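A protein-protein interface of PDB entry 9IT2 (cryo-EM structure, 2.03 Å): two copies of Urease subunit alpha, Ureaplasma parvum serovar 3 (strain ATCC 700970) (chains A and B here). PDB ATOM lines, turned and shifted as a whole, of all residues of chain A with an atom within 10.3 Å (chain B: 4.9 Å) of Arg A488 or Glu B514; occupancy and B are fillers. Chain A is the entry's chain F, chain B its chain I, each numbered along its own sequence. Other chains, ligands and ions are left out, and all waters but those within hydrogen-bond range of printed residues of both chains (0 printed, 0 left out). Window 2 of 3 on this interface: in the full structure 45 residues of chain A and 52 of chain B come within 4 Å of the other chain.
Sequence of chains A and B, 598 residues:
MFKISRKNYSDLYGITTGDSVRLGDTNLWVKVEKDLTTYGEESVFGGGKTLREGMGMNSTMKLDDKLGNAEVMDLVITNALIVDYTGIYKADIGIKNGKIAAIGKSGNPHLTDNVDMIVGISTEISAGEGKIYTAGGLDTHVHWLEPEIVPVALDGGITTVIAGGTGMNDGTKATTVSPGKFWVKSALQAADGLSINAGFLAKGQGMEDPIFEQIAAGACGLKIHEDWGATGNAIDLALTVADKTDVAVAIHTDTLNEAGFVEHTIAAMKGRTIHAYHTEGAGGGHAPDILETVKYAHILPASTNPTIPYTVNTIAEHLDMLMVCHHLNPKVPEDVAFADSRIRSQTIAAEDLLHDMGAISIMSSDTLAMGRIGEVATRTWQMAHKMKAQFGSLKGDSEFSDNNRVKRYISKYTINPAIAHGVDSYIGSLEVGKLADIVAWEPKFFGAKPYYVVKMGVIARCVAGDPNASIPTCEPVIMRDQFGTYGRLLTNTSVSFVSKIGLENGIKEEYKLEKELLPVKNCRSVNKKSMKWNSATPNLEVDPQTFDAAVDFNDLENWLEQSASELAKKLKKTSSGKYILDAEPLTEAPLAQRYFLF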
ATOM      1  N   ASP A 192     -11.095  10.824  13.410  1.00  0.00           N
ATOM      2  CA  ASP A 192      -9.781  11.122  12.850  1.00  0.00           C
ATOM      3  C   ASP A 192      -9.796  12.396  12.013  1.00  0.00           C
ATOM      4  O   ASP A 192      -8.756  13.044  11.854  1.00  0.00           O
ATOM      5  CB  ASP A 192      -9.296   9.939  12.010  1.00  0.00           C
ATOM      6  CG  ASP A 192      -7.800   9.719  12.119  1.00  0.00           C
ATOM      7  OD1 ASP A 192      -7.297   9.573  13.252  1.00  0.00           O
ATOM      8  OD2 ASP A 192      -7.126   9.684  11.069  1.00  0.00           O
ATOM      9  N   GLY A 193     -10.954  12.770  11.473  1.00  0.00           N
ATOM     10  CA  GLY A 193     -11.067  13.985  10.691  1.00  0.00           C
ATOM     11  C   GLY A 193     -11.895  15.069  11.353  1.00  0.00           C
ATOM     12  O   GLY A 193     -12.584  15.834  10.670  1.00  0.00           O
ATOM     13  N   LEU A 194     -11.842  15.144  12.682  1.00  0.00           N
ATOM     14  CA  LEU A 194     -12.518  16.186  13.442  1.00  0.00           C
ATOM     15  C   LEU A 194     -11.570  16.736  14.498  1.00  0.00           C
ATOM     16  O   LEU A 194     -10.717  16.016  15.022  1.00  0.00           O
ATOM     17  CB  LEU A 194     -13.800  15.662  14.101  1.00  0.00           C
ATOM     18  CG  LEU A 194     -14.936  15.281  13.148  1.00  0.00           C
ATOM     19  CD1 LEU A 194     -15.822  14.210  13.763  1.00  0.00           C
ATOM     20  CD2 LEU A 194     -15.755  16.503  12.764  1.00  0.00           C
ATOM     21  N   SER A 195     -11.731  18.023  14.810  1.00  0.00           N
ATOM     22  CA  SER A 195     -10.828  18.716  15.732  1.00  0.00           C
ATOM     23  C   SER A 195     -11.403  18.657  17.145  1.00  0.00           C
ATOM     24  O   SER A 195     -11.925  19.634  17.686  1.00  0.00           O
ATOM     25  CB  SER A 195     -10.598  20.151  15.277  1.00  0.00           C
ATOM     26  OG  SER A 195     -11.690  20.982  15.628  1.00  0.00           O
ATOM     27  N   LYS A 455      -6.101  23.645  21.120  1.00  0.00           N
ATOM     28  CA  LYS A 455      -5.975  22.192  21.153  1.00  0.00           C
ATOM     29  C   LYS A 455      -4.505  21.838  20.967  1.00  0.00           C
ATOM     30  O   LYS A 455      -3.966  21.968  19.862  1.00  0.00           O
ATOM     31  CB  LYS A 455      -6.838  21.549  20.069  1.00  0.00           C
ATOM     32  CG  LYS A 455      -8.310  21.436  20.426  1.00  0.00           C
ATOM     33  CD  LYS A 455      -8.521  20.533  21.628  1.00  0.00           C
ATOM     34  CE  LYS A 455      -8.383  19.068  21.246  1.00  0.00           C
ATOM     35  NZ  LYS A 455      -7.012  18.548  21.509  1.00  0.00           N
ATOM     36  N   MET A 456      -3.864  21.389  22.047  1.00  0.00           N
ATOM     37  CA  MET A 456      -2.450  21.008  22.039  1.00  0.00           C
ATOM     38  C   MET A 456      -1.571  22.145  21.519  1.00  0.00           C
ATOM     39  O   MET A 456      -0.710  21.959  20.657  1.00  0.00           O
ATOM     40  CB  MET A 456      -2.233  19.726  21.232  1.00  0.00           C
ATOM     41  CG  MET A 456      -3.094  18.559  21.688  1.00  0.00           C
ATOM     42  SD  MET A 456      -2.686  16.996  20.886  1.00  0.00           S
ATOM     43  CE  MET A 456      -0.955  16.832  21.311  1.00  0.00           C
ATOM     44  N   VAL A 458      -2.361  24.751  19.716  1.00  0.00           N
ATOM     45  CA  VAL A 458      -2.765  25.350  18.451  1.00  0.00           C
ATOM     46  C   VAL A 458      -4.241  25.711  18.538  1.00  0.00           C
ATOM     47  O   VAL A 458      -5.053  24.912  19.018  1.00  0.00           O
ATOM     48  CB  VAL A 458      -2.500  24.404  17.265  1.00  0.00           C
ATOM     49  CG1 VAL A 458      -2.954  25.039  15.957  1.00  0.00           C
ATOM     50  CG2 VAL A 458      -1.026  24.033  17.204  1.00  0.00           C
ATOM     51  N   GLN A 482     -10.139  27.371  12.706  1.00  0.00           N
ATOM     52  CA  GLN A 482      -8.803  27.911  12.530  1.00  0.00           C
ATOM     53  C   GLN A 482      -7.897  26.868  11.874  1.00  0.00           C
ATOM     54  O   GLN A 482      -8.354  25.804  11.441  1.00  0.00           O
ATOM     55  CB  GLN A 482      -8.266  28.393  13.878  1.00  0.00           C
ATOM     56  CG  GLN A 482      -9.057  29.560  14.445  1.00  0.00           C
ATOM     57  CD  GLN A 482      -9.160  30.720  13.472  1.00  0.00           C
ATOM     58  OE1 GLN A 482      -8.151  31.220  12.978  1.00  0.00           O
ATOM     59  NE2 GLN A 482     -10.384  31.148  13.189  1.00  0.00           N
ATOM     60  N   PHE A 483      -6.602  27.187  11.791  1.00  0.00           N
ATOM     61  CA  PHE A 483      -5.651  26.304  11.124  1.00  0.00           C
ATOM     62  C   PHE A 483      -5.541  24.945  11.800  1.00  0.00           C
ATOM     63  O   PHE A 483      -5.118  23.978  11.157  1.00  0.00           O
ATOM     64  CB  PHE A 483      -4.272  26.962  11.063  1.00  0.00           C
ATOM     65  CG  PHE A 483      -4.240  28.220  10.250  1.00  0.00           C
ATOM     66  CD1 PHE A 483      -4.409  28.177   8.876  1.00  0.00           C
ATOM     67  CD2 PHE A 483      -4.037  29.448  10.856  1.00  0.00           C
ATOM     68  CE1 PHE A 483      -4.383  29.334   8.125  1.00  0.00           C
ATOM     69  CE2 PHE A 483      -4.005  30.609  10.107  1.00  0.00           C
ATOM     70  CZ  PHE A 483      -4.176  30.551   8.740  1.00  0.00           C
ATOM     71  N   GLY A 484      -5.917  24.843  13.075  1.00  0.00           N
ATOM     72  CA  GLY A 484      -5.879  23.568  13.769  1.00  0.00           C
ATOM     73  C   GLY A 484      -6.826  22.527  13.212  1.00  0.00           C
ATOM     74  O   GLY A 484      -6.727  21.356  13.594  1.00  0.00           O
ATOM     75  N   THR A 485      -7.744  22.921  12.331  1.00  0.00           N
ATOM     76  CA  THR A 485      -8.687  22.004  11.708  1.00  0.00           C
ATOM     77  C   THR A 485      -8.321  21.665  10.267  1.00  0.00           C
ATOM     78  O   THR A 485      -9.139  21.074   9.557  1.00  0.00           O
ATOM     79  CB  THR A 485     -10.100  22.590  11.758  1.00  0.00           C
ATOM     80  OG1 THR A 485     -10.200  23.680  10.833  1.00  0.00           O
ATOM     81  CG2 THR A 485     -10.418  23.096  13.154  1.00  0.00           C
ATOM     82  N   TYR A 486      -7.119  22.023   9.818  1.00  0.00           N
ATOM     83  CA  TYR A 486      -6.731  21.860   8.424  1.00  0.00           C
ATOM     84  C   TYR A 486      -5.464  21.023   8.301  1.00  0.00           C
ATOM     85  O   TYR A 486      -4.577  21.073   9.159  1.00  0.00           O
ATOM     86  CB  TYR A 486      -6.506  23.220   7.751  1.00  0.00           C
ATOM     87  CG  TYR A 486      -7.777  23.911   7.319  1.00  0.00           C
ATOM     88  CD1 TYR A 486      -8.497  24.698   8.206  1.00  0.00           C
ATOM     89  CD2 TYR A 486      -8.254  23.781   6.022  1.00  0.00           C
ATOM     90  CE1 TYR A 486      -9.659  25.331   7.816  1.00  0.00           C
ATOM     91  CE2 TYR A 486      -9.415  24.412   5.622  1.00  0.00           C
ATOM     92  CZ  TYR A 486     -10.113  25.186   6.524  1.00  0.00           C
ATOM     93  OH  TYR A 486     -11.271  25.817   6.131  1.00  0.00           O
ATOM     94  N   GLY A 487      -5.393  20.258   7.213  1.00  0.00           N
ATOM     95  CA  GLY A 487      -4.181  19.531   6.866  1.00  0.00           C
ATOM     96  C   GLY A 487      -3.801  18.502   7.910  1.00  0.00           C
ATOM     97  O   GLY A 487      -4.653  17.866   8.538  1.00  0.00           O
ATOM     98  N   ARG A 488      -2.491  18.327   8.092  1.00  0.00           N
ATOM     99  CA  ARG A 488      -1.979  17.434   9.123  1.00  0.00           C
ATOM    100  C   ARG A 488      -2.075  18.041  10.514  1.00  0.00           C
ATOM    101  O   ARG A 488      -1.997  17.308  11.507  1.00  0.00           O
ATOM    102  CB  ARG A 488      -0.528  17.056   8.819  1.00  0.00           C
ATOM    103  CG  ARG A 488      -0.194  16.995   7.332  1.00  0.00           C
ATOM    104  CD  ARG A 488      -0.676  15.702   6.682  1.00  0.00           C
ATOM    105  NE  ARG A 488      -2.119  15.679   6.477  1.00  0.00           N
ATOM    106  CZ  ARG A 488      -2.733  16.145   5.399  1.00  0.00           C
ATOM    107  NH1 ARG A 488      -2.056  16.681   4.396  1.00  0.00           N
ATOM    108  NH2 ARG A 488      -4.058  16.074   5.325  1.00  0.00           N
ATOM    109  N   LEU A 489      -2.237  19.363  10.603  1.00  0.00           N
ATOM    110  CA  LEU A 489      -2.455  19.999  11.896  1.00  0.00           C
ATOM    111  C   LEU A 489      -3.733  19.496  12.551  1.00  0.00           C
ATOM    112  O   LEU A 489      -3.828  19.463  13.783  1.00  0.00           O
ATOM    113  CB  LEU A 489      -2.499  21.519  11.728  1.00  0.00           C
ATOM    114  CG  LEU A 489      -1.902  22.358  12.856  1.00  0.00           C
ATOM    115  CD1 LEU A 489      -0.509  21.860  13.215  1.00  0.00           C
ATOM    116  CD2 LEU A 489      -1.870  23.830  12.466  1.00  0.00           C
ATOM    117  N   LEU A 490      -4.724  19.101  11.747  1.00  0.00           N
ATOM    118  CA  LEU A 490      -5.953  18.543  12.298  1.00  0.00           C
ATOM    119  C   LEU A 490      -5.682  17.246  13.053  1.00  0.00           C
ATOM    120  O   LEU A 490      -6.229  17.026  14.139  1.00  0.00           O
ATOM    121  CB  LEU A 490      -6.970  18.313  11.179  1.00  0.00           C
ATOM    122  CG  LEU A 490      -8.207  17.481  11.524  1.00  0.00           C
ATOM    123  CD1 LEU A 490      -9.185  18.291  12.360  1.00  0.00           C
ATOM    124  CD2 LEU A 490      -8.878  16.965  10.260  1.00  0.00           C
ATOM    125  N   THR A 491      -4.838  16.379  12.497  1.00  0.00           N
ATOM    126  CA  THR A 491      -4.509  15.113  13.136  1.00  0.00           C
ATOM    127  C   THR A 491      -3.351  15.223  14.117  1.00  0.00           C
ATOM    128  O   THR A 491      -3.058  14.247  14.815  1.00  0.00           O
ATOM    129  CB  THR A 491      -4.176  14.054  12.078  1.00  0.00           C
ATOM    130  OG1 THR A 491      -3.069  14.498  11.285  1.00  0.00           O
ATOM    131  CG2 THR A 491      -5.376  13.805  11.176  1.00  0.00           C
ATOM    132  N   ASN A 492      -2.689  16.377  14.188  1.00  0.00           N
ATOM    133  CA  ASN A 492      -1.620  16.590  15.155  1.00  0.00           C
ATOM    134  C   ASN A 492      -2.083  17.253  16.445  1.00  0.00           C
ATOM    135  O   ASN A 492      -1.401  17.121  17.467  1.00  0.00           O
ATOM    136  CB  ASN A 492      -0.503  17.442  14.541  1.00  0.00           C
ATOM    137  CG  ASN A 492       0.488  16.623  13.744  1.00  0.00           C
ATOM    138  OD1 ASN A 492       1.202  17.149  12.895  1.00  0.00           O
ATOM    139  ND2 ASN A 492       0.537  15.325  14.014  1.00  0.00           N
ATOM    140  N   THR A 493      -3.213  17.959  16.430  1.00  0.00           N
ATOM    141  CA  THR A 493      -3.634  18.782  17.557  1.00  0.00           C
ATOM    142  C   THR A 493      -4.746  18.148  18.384  1.00  0.00           C
ATOM    143  O   THR A 493      -5.284  18.803  19.282  1.00  0.00           O
ATOM    144  CB  THR A 493      -4.071  20.164  17.067  1.00  0.00           C
ATOM    145  OG1 THR A 493      -5.069  20.024  16.047  1.00  0.00           O
ATOM    146  CG2 THR A 493      -2.880  20.918  16.502  1.00  0.00           C
ATOM    147  N   SER A 494      -5.105  16.897  18.109  1.00  0.00           N
ATOM    148  CA  SER A 494      -6.070  16.186  18.934  1.00  0.00           C
ATOM    149  C   SER A 494      -5.722  14.706  18.921  1.00  0.00           C
ATOM    150  O   SER A 494      -4.975  14.231  18.062  1.00  0.00           O
ATOM    151  CB  SER A 494      -7.511  16.418  18.461  1.00  0.00           C
ATOM    152  OG  SER A 494      -7.647  16.174  17.075  1.00  0.00           O
ATOM    153  N   VAL A 495      -6.273  13.978  19.892  1.00  0.00           N
ATOM    154  CA  VAL A 495      -5.966  12.570  20.089  1.00  0.00           C
ATOM    155  C   VAL A 495      -7.268  11.781  20.144  1.00  0.00           C
ATOM    156  O   VAL A 495      -8.361  12.340  20.237  1.00  0.00           O
ATOM    157  CB  VAL A 495      -5.139  12.323  21.368  1.00  0.00           C
ATOM    158  CG1 VAL A 495      -3.766  12.972  21.254  1.00  0.00           C
ATOM    159  CG2 VAL A 495      -5.884  12.835  22.594  1.00  0.00           C
ATOM    160  N   LYS A 512      -6.107   2.453   9.896  1.00  0.00           N
ATOM    161  CA  LYS A 512      -5.467   3.507   9.106  1.00  0.00           C
ATOM    162  C   LYS A 512      -5.683   4.879   9.738  1.00  0.00           C
ATOM    163  O   LYS A 512      -5.936   5.868   9.049  1.00  0.00           O
ATOM    164  CB  LYS A 512      -5.959   3.487   7.657  1.00  0.00           C
ATOM    165  CG  LYS A 512      -5.674   2.186   6.926  1.00  0.00           C
ATOM    166  CD  LYS A 512      -5.884   2.337   5.429  1.00  0.00           C
ATOM    167  CE  LYS A 512      -5.992   0.984   4.746  1.00  0.00           C
ATOM    168  NZ  LYS A 512      -7.285   0.831   4.022  1.00  0.00           N
ATOM    169  N   GLU A 514      -4.738   8.367  11.664  1.00  0.00           N
ATOM    170  CA  GLU A 514      -3.635   9.315  11.623  1.00  0.00           C
ATOM    171  C   GLU A 514      -3.382  10.008  12.955  1.00  0.00           C
ATOM    172  O   GLU A 514      -2.286  10.538  13.159  1.00  0.00           O
ATOM    173  CB  GLU A 514      -3.886  10.372  10.540  1.00  0.00           C
ATOM    174  CG  GLU A 514      -3.698   9.850   9.123  1.00  0.00           C
ATOM    175  CD  GLU A 514      -4.423  10.685   8.087  1.00  0.00           C
ATOM    176  OE1 GLU A 514      -4.784  11.840   8.395  1.00  0.00           O
ATOM    177  OE2 GLU A 514      -4.633  10.185   6.962  1.00  0.00           O
ATOM    178  N   LYS A 515      -4.357  10.012  13.860  1.00  0.00           N
ATOM    179  CA  LYS A 515      -4.174  10.635  15.160  1.00  0.00           C
ATOM    180  C   LYS A 515      -3.382   9.725  16.094  1.00  0.00           C
ATOM    181  O   LYS A 515      -3.321   8.506  15.919  1.00  0.00           O
ATOM    182  CB  LYS A 515      -5.522  10.967  15.799  1.00  0.00           C
ATOM    183  CG  LYS A 515      -6.202  12.200  15.243  1.00  0.00           C
ATOM    184  CD  LYS A 515      -7.478  12.502  16.010  1.00  0.00           C
ATOM    185  CE  LYS A 515      -8.270  13.614  15.349  1.00  0.00           C
ATOM    186  NZ  LYS A 515      -9.343  14.129  16.241  1.00  0.00           N
ATOM    187  N   GLU A 516      -2.765  10.342  17.098  1.00  0.00           N
ATOM    188  CA  GLU A 516      -2.154   9.584  18.178  1.00  0.00           C
ATOM    189  C   GLU A 516      -3.238   8.977  19.062  1.00  0.00           C
ATOM    190  O   GLU A 516      -4.239   9.626  19.378  1.00  0.00           O
ATOM    191  CB  GLU A 516      -1.235  10.481  19.006  1.00  0.00           C
ATOM    192  CG  GLU A 516      -0.655   9.809  20.243  1.00  0.00           C
ATOM    193  CD  GLU A 516       0.320  10.696  20.992  1.00  0.00           C
ATOM    194  OE1 GLU A 516       0.092  11.923  21.045  1.00  0.00           O
ATOM    195  OE2 GLU A 516       1.316  10.166  21.528  1.00  0.00           O
ATOM    196  N   GLN B 189       2.046  22.240   7.790  1.00  0.00           N
ATOM    197  CA  GLN B 189       1.041  21.191   7.913  1.00  0.00           C
ATOM    198  C   GLN B 189      -0.359  21.729   7.641  1.00  0.00           C
ATOM    199  O   GLN B 189      -1.169  21.061   6.989  1.00  0.00           O
ATOM    200  CB  GLN B 189       1.119  20.553   9.300  1.00  0.00           C
ATOM    201  CG  GLN B 189       2.255  19.555   9.449  1.00  0.00           C
ATOM    202  CD  GLN B 189       2.469  19.118  10.884  1.00  0.00           C
ATOM    203  OE1 GLN B 189       2.076  19.809  11.820  1.00  0.00           O
ATOM    204  NE2 GLN B 189       3.094  17.961  11.060  1.00  0.00           N
ATOM    205  N   ASP B 192      -0.818  22.328   3.999  1.00  0.00           N
ATOM    206  CA  ASP B 192      -0.974  21.081   3.259  1.00  0.00           C
ATOM    207  C   ASP B 192      -2.430  20.793   2.915  1.00  0.00           C
ATOM    208  O   ASP B 192      -2.693  20.042   1.970  1.00  0.00           O
ATOM    209  CB  ASP B 192      -0.386  19.921   4.067  1.00  0.00           C
ATOM    210  CG  ASP B 192       0.268  18.871   3.190  1.00  0.00           C
ATOM    211  OD1 ASP B 192       1.096  19.239   2.331  1.00  0.00           O
ATOM    212  OD2 ASP B 192      -0.040  17.675   3.365  1.00  0.00           O
ATOM    213  N   THR B 491      -3.672  18.336  -2.886  1.00  0.00           N
ATOM    214  CA  THR B 491      -2.235  18.264  -2.667  1.00  0.00           C
ATOM    215  C   THR B 491      -1.448  18.065  -3.955  1.00  0.00           C
ATOM    216  O   THR B 491      -0.218  17.968  -3.905  1.00  0.00           O
ATOM    217  CB  THR B 491      -1.903  17.136  -1.683  1.00  0.00           C
ATOM    218  OG1 THR B 491      -2.370  15.887  -2.206  1.00  0.00           O
ATOM    219  CG2 THR B 491      -2.560  17.393  -0.333  1.00  0.00           C
ATOM    220  N   LYS B 508       9.818  17.092   4.619  1.00  0.00           N
ATOM    221  CA  LYS B 508       8.595  16.565   4.020  1.00  0.00           C
ATOM    222  C   LYS B 508       8.181  15.253   4.673  1.00  0.00           C
ATOM    223  O   LYS B 508       7.001  15.050   4.981  1.00  0.00           O
ATOM    224  CB  LYS B 508       8.788  16.373   2.516  1.00  0.00           C
ATOM    225  CG  LYS B 508       7.587  15.770   1.806  1.00  0.00           C
ATOM    226  CD  LYS B 508       7.726  15.875   0.298  1.00  0.00           C
ATOM    227  CE  LYS B 508       6.787  14.916  -0.413  1.00  0.00           C
ATOM    228  NZ  LYS B 508       5.359  15.202  -0.107  1.00  0.00           N
ATOM    229  N   TYR B 511       7.525  16.007   8.667  1.00  0.00           N
ATOM    230  CA  TYR B 511       6.260  16.689   8.898  1.00  0.00           C
ATOM    231  C   TYR B 511       5.078  15.963   8.272  1.00  0.00           C
ATOM    232  O   TYR B 511       3.939  16.418   8.427  1.00  0.00           O
ATOM    233  CB  TYR B 511       6.320  18.127   8.367  1.00  0.00           C
ATOM    234  CG  TYR B 511       7.427  18.974   8.961  1.00  0.00           C
ATOM    235  CD1 TYR B 511       8.060  18.602  10.141  1.00  0.00           C
ATOM    236  CD2 TYR B 511       7.836  20.147   8.341  1.00  0.00           C
ATOM    237  CE1 TYR B 511       9.068  19.371  10.685  1.00  0.00           C
ATOM    238  CE2 TYR B 511       8.844  20.924   8.879  1.00  0.00           C
ATOM    239  CZ  TYR B 511       9.457  20.531  10.049  1.00  0.00           C
ATOM    240  OH  TYR B 511      10.461  21.298  10.589  1.00  0.00           O
ATOM    241  N   LYS B 512       5.324  14.849   7.578  1.00  0.00           N
ATOM    242  CA  LYS B 512       4.279  14.077   6.906  1.00  0.00           C
ATOM    243  C   LYS B 512       3.502  14.940   5.916  1.00  0.00           C
ATOM    244  O   LYS B 512       2.275  14.870   5.829  1.00  0.00           O
ATOM    245  CB  LYS B 512       3.334  13.424   7.918  1.00  0.00           C
ATOM    246  CG  LYS B 512       4.016  12.457   8.871  1.00  0.00           C
ATOM    247  CD  LYS B 512       3.034  11.911   9.893  1.00  0.00           C
ATOM    248  CE  LYS B 512       3.744  11.111  10.972  1.00  0.00           C
ATOM    249  NZ  LYS B 512       2.947  11.047  12.228  1.00  0.00           N
ATOM    250  N   LEU B 513       4.224  15.762   5.161  1.00  0.00           N
ATOM    251  CA  LEU B 513       3.599  16.642   4.186  1.00  0.00           C
ATOM    252  C   LEU B 513       3.283  15.880   2.906  1.00  0.00           C
ATOM    253  O   LEU B 513       4.101  15.099   2.411  1.00  0.00           O
ATOM    254  CB  LEU B 513       4.510  17.830   3.879  1.00  0.00           C
ATOM    255  CG  LEU B 513       4.758  18.795   5.040  1.00  0.00           C
ATOM    256  CD1 LEU B 513       5.689  19.921   4.616  1.00  0.00           C
ATOM    257  CD2 LEU B 513       3.443  19.347   5.575  1.00  0.00           C
ATOM    258  N   GLU B 514       2.086  16.111   2.371  1.00  0.00           N
ATOM    259  CA  GLU B 514       1.660  15.453   1.145  1.00  0.00           C
ATOM    260  C   GLU B 514       1.918  16.287  -0.100  1.00  0.00           C
ATOM    261  O   GLU B 514       1.936  15.735  -1.207  1.00  0.00           O
ATOM    262  CB  GLU B 514       0.173  15.097   1.231  1.00  0.00           C
ATOM    263  CG  GLU B 514      -0.129  13.991   2.231  1.00  0.00           C
ATOM    264  CD  GLU B 514      -1.584  13.962   2.656  1.00  0.00           C
ATOM    265  OE1 GLU B 514      -2.434  14.492   1.910  1.00  0.00           O
ATOM    266  OE2 GLU B 514      -1.876  13.412   3.738  1.00  0.00           O
ATOM    267  N   LYS B 515       2.120  17.593   0.047  1.00  0.00           N
ATOM    268  CA  LYS B 515       2.399  18.449  -1.093  1.00  0.00           C
ATOM    269  C   LYS B 515       3.860  18.334  -1.513  1.00  0.00           C
ATOM    270  O   LYS B 515       4.731  17.933  -0.736  1.00  0.00           O
ATOM    271  CB  LYS B 515       2.073  19.906  -0.769  1.00  0.00           C
ATOM    272  CG  LYS B 515       0.597  20.244  -0.796  1.00  0.00           C
ATOM    273  CD  LYS B 515       0.378  21.731  -0.581  1.00  0.00           C
ATOM    274  CE  LYS B 515      -1.092  22.046  -0.387  1.00  0.00           C
ATOM    275  NZ  LYS B 515      -1.360  23.507  -0.489  1.00  0.00           N
ATOM    276  N   GLU B 516       4.119  18.688  -2.768  1.00  0.00           N
ATOM    277  CA  GLU B 516       5.489  18.827  -3.237  1.00  0.00           C
ATOM    278  C   GLU B 516       6.114  20.085  -2.646  1.00  0.00           C
ATOM    279  O   GLU B 516       5.463  21.127  -2.536  1.00  0.00           O
ATOM    280  CB  GLU B 516       5.525  18.879  -4.765  1.00  0.00           C
ATOM    281  CG  GLU B 516       6.843  19.370  -5.350  1.00  0.00           C
ATOM    282  CD  GLU B 516       6.927  19.179  -6.851  1.00  0.00           C
ATOM    283  OE1 GLU B 516       6.020  19.656  -7.565  1.00  0.00           O
ATOM    284  OE2 GLU B 516       7.901  18.554  -7.318  1.00  0.00           O
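The backbone NH (N) of Arg A488 sits at hydrogen-bond distance from the backbone carbonyl oxygen (O) of Gln B189 (3.2 Å).
The guanidinium group (NH1) of Arg A488 lies within salt-bridge range of the side-chain carboxylate (OD2) of Asp B192.
NH1 of Arg A488 is in salt-bridge range of OE1 of Glu B514.
The side-chain amide nitrogen (NE2) of Gln B189 lies within hydrogen-bond range of the side-chain amide oxygen (OD1) of Asn A492.
The side-chain hydroxyl (OG1) of Thr A491 sits at hydrogen-bond distance from the backbone carbonyl oxygen (O) of Arg A488 (3.0 Å).
O of Arg A488 lies close to OD1 of Asn A492.
The backbone carbonyl oxygen (O) of Leu A489 is in hydrogen-bond range of the side-chain hydroxyl (OG1) of Thr A493 (2.6 Å).
The side-chain amide nitrogen (NE2) of Gln B189 lies within hydrogen-bond range of the backbone carbonyl oxygen (O) of Tyr B511, at 3.2 Å.
OD2 of Asp B192 lies within hydrogen-bond range of N of Glu B514.
OD1 of Asp B192 is in hydrogen-bond range of N of Lys B515.
Gly A487 touches Gln B189.
CD of Arg A488 touches O of Lys B512, at 3.2 Å.
Gln B189 touches Leu A489 (OE1 to CD1, 3.6 Å).
Val A458 touches none of the printed residues of chain B.
Tyr A486 touches none of the printed residues of chain B.
Of chain B, only Gln B189 (3.2 Å), Asp B192 (2.5 Å), Lys B512 (3.2 Å) and Glu B514 (3.3 Å) come within 4 Å of Arg A488.
Of the printed residues of chain B, Asn A492 touches Gln B189 (2.8 Å).
Gln B189 touches just these residues of chain A: Gly A487, Arg A488, Leu A489 and Asn A492.
Of chain A, only Arg A488 comes within 4 Å of Asp B192.
Of the printed residues of chain A, Lys B512 touches Arg A488.
Glu B514 touches one residue of chain A.
Hydrophobic or aromatic side chains of chain A within 4 Å of the printed part of chain B: Leu A489.
Of the 10 printed residues of chain B, 4 touch a printed residue of chain A.
Printed residues of chain B that touch a printed residue of chain A: Gln B189, Asp B192, Lys B512 and Glu B514.
Among the printed residues, 7 pairs touch across the chains.
Among the printed residues, Asp or Glu carboxylates within 4 Å of a Lys or Arg side-chain nitrogen of the other chain: Arg A488 with Asp B192 and Arg A488 with Glu B514.
Positions printed for both chains: 192, 491, 512, 514, 515 and 516.
Of the 7 pairs that touch across the chains among the printed residues, none has its exchanged pair printed and touching as well.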
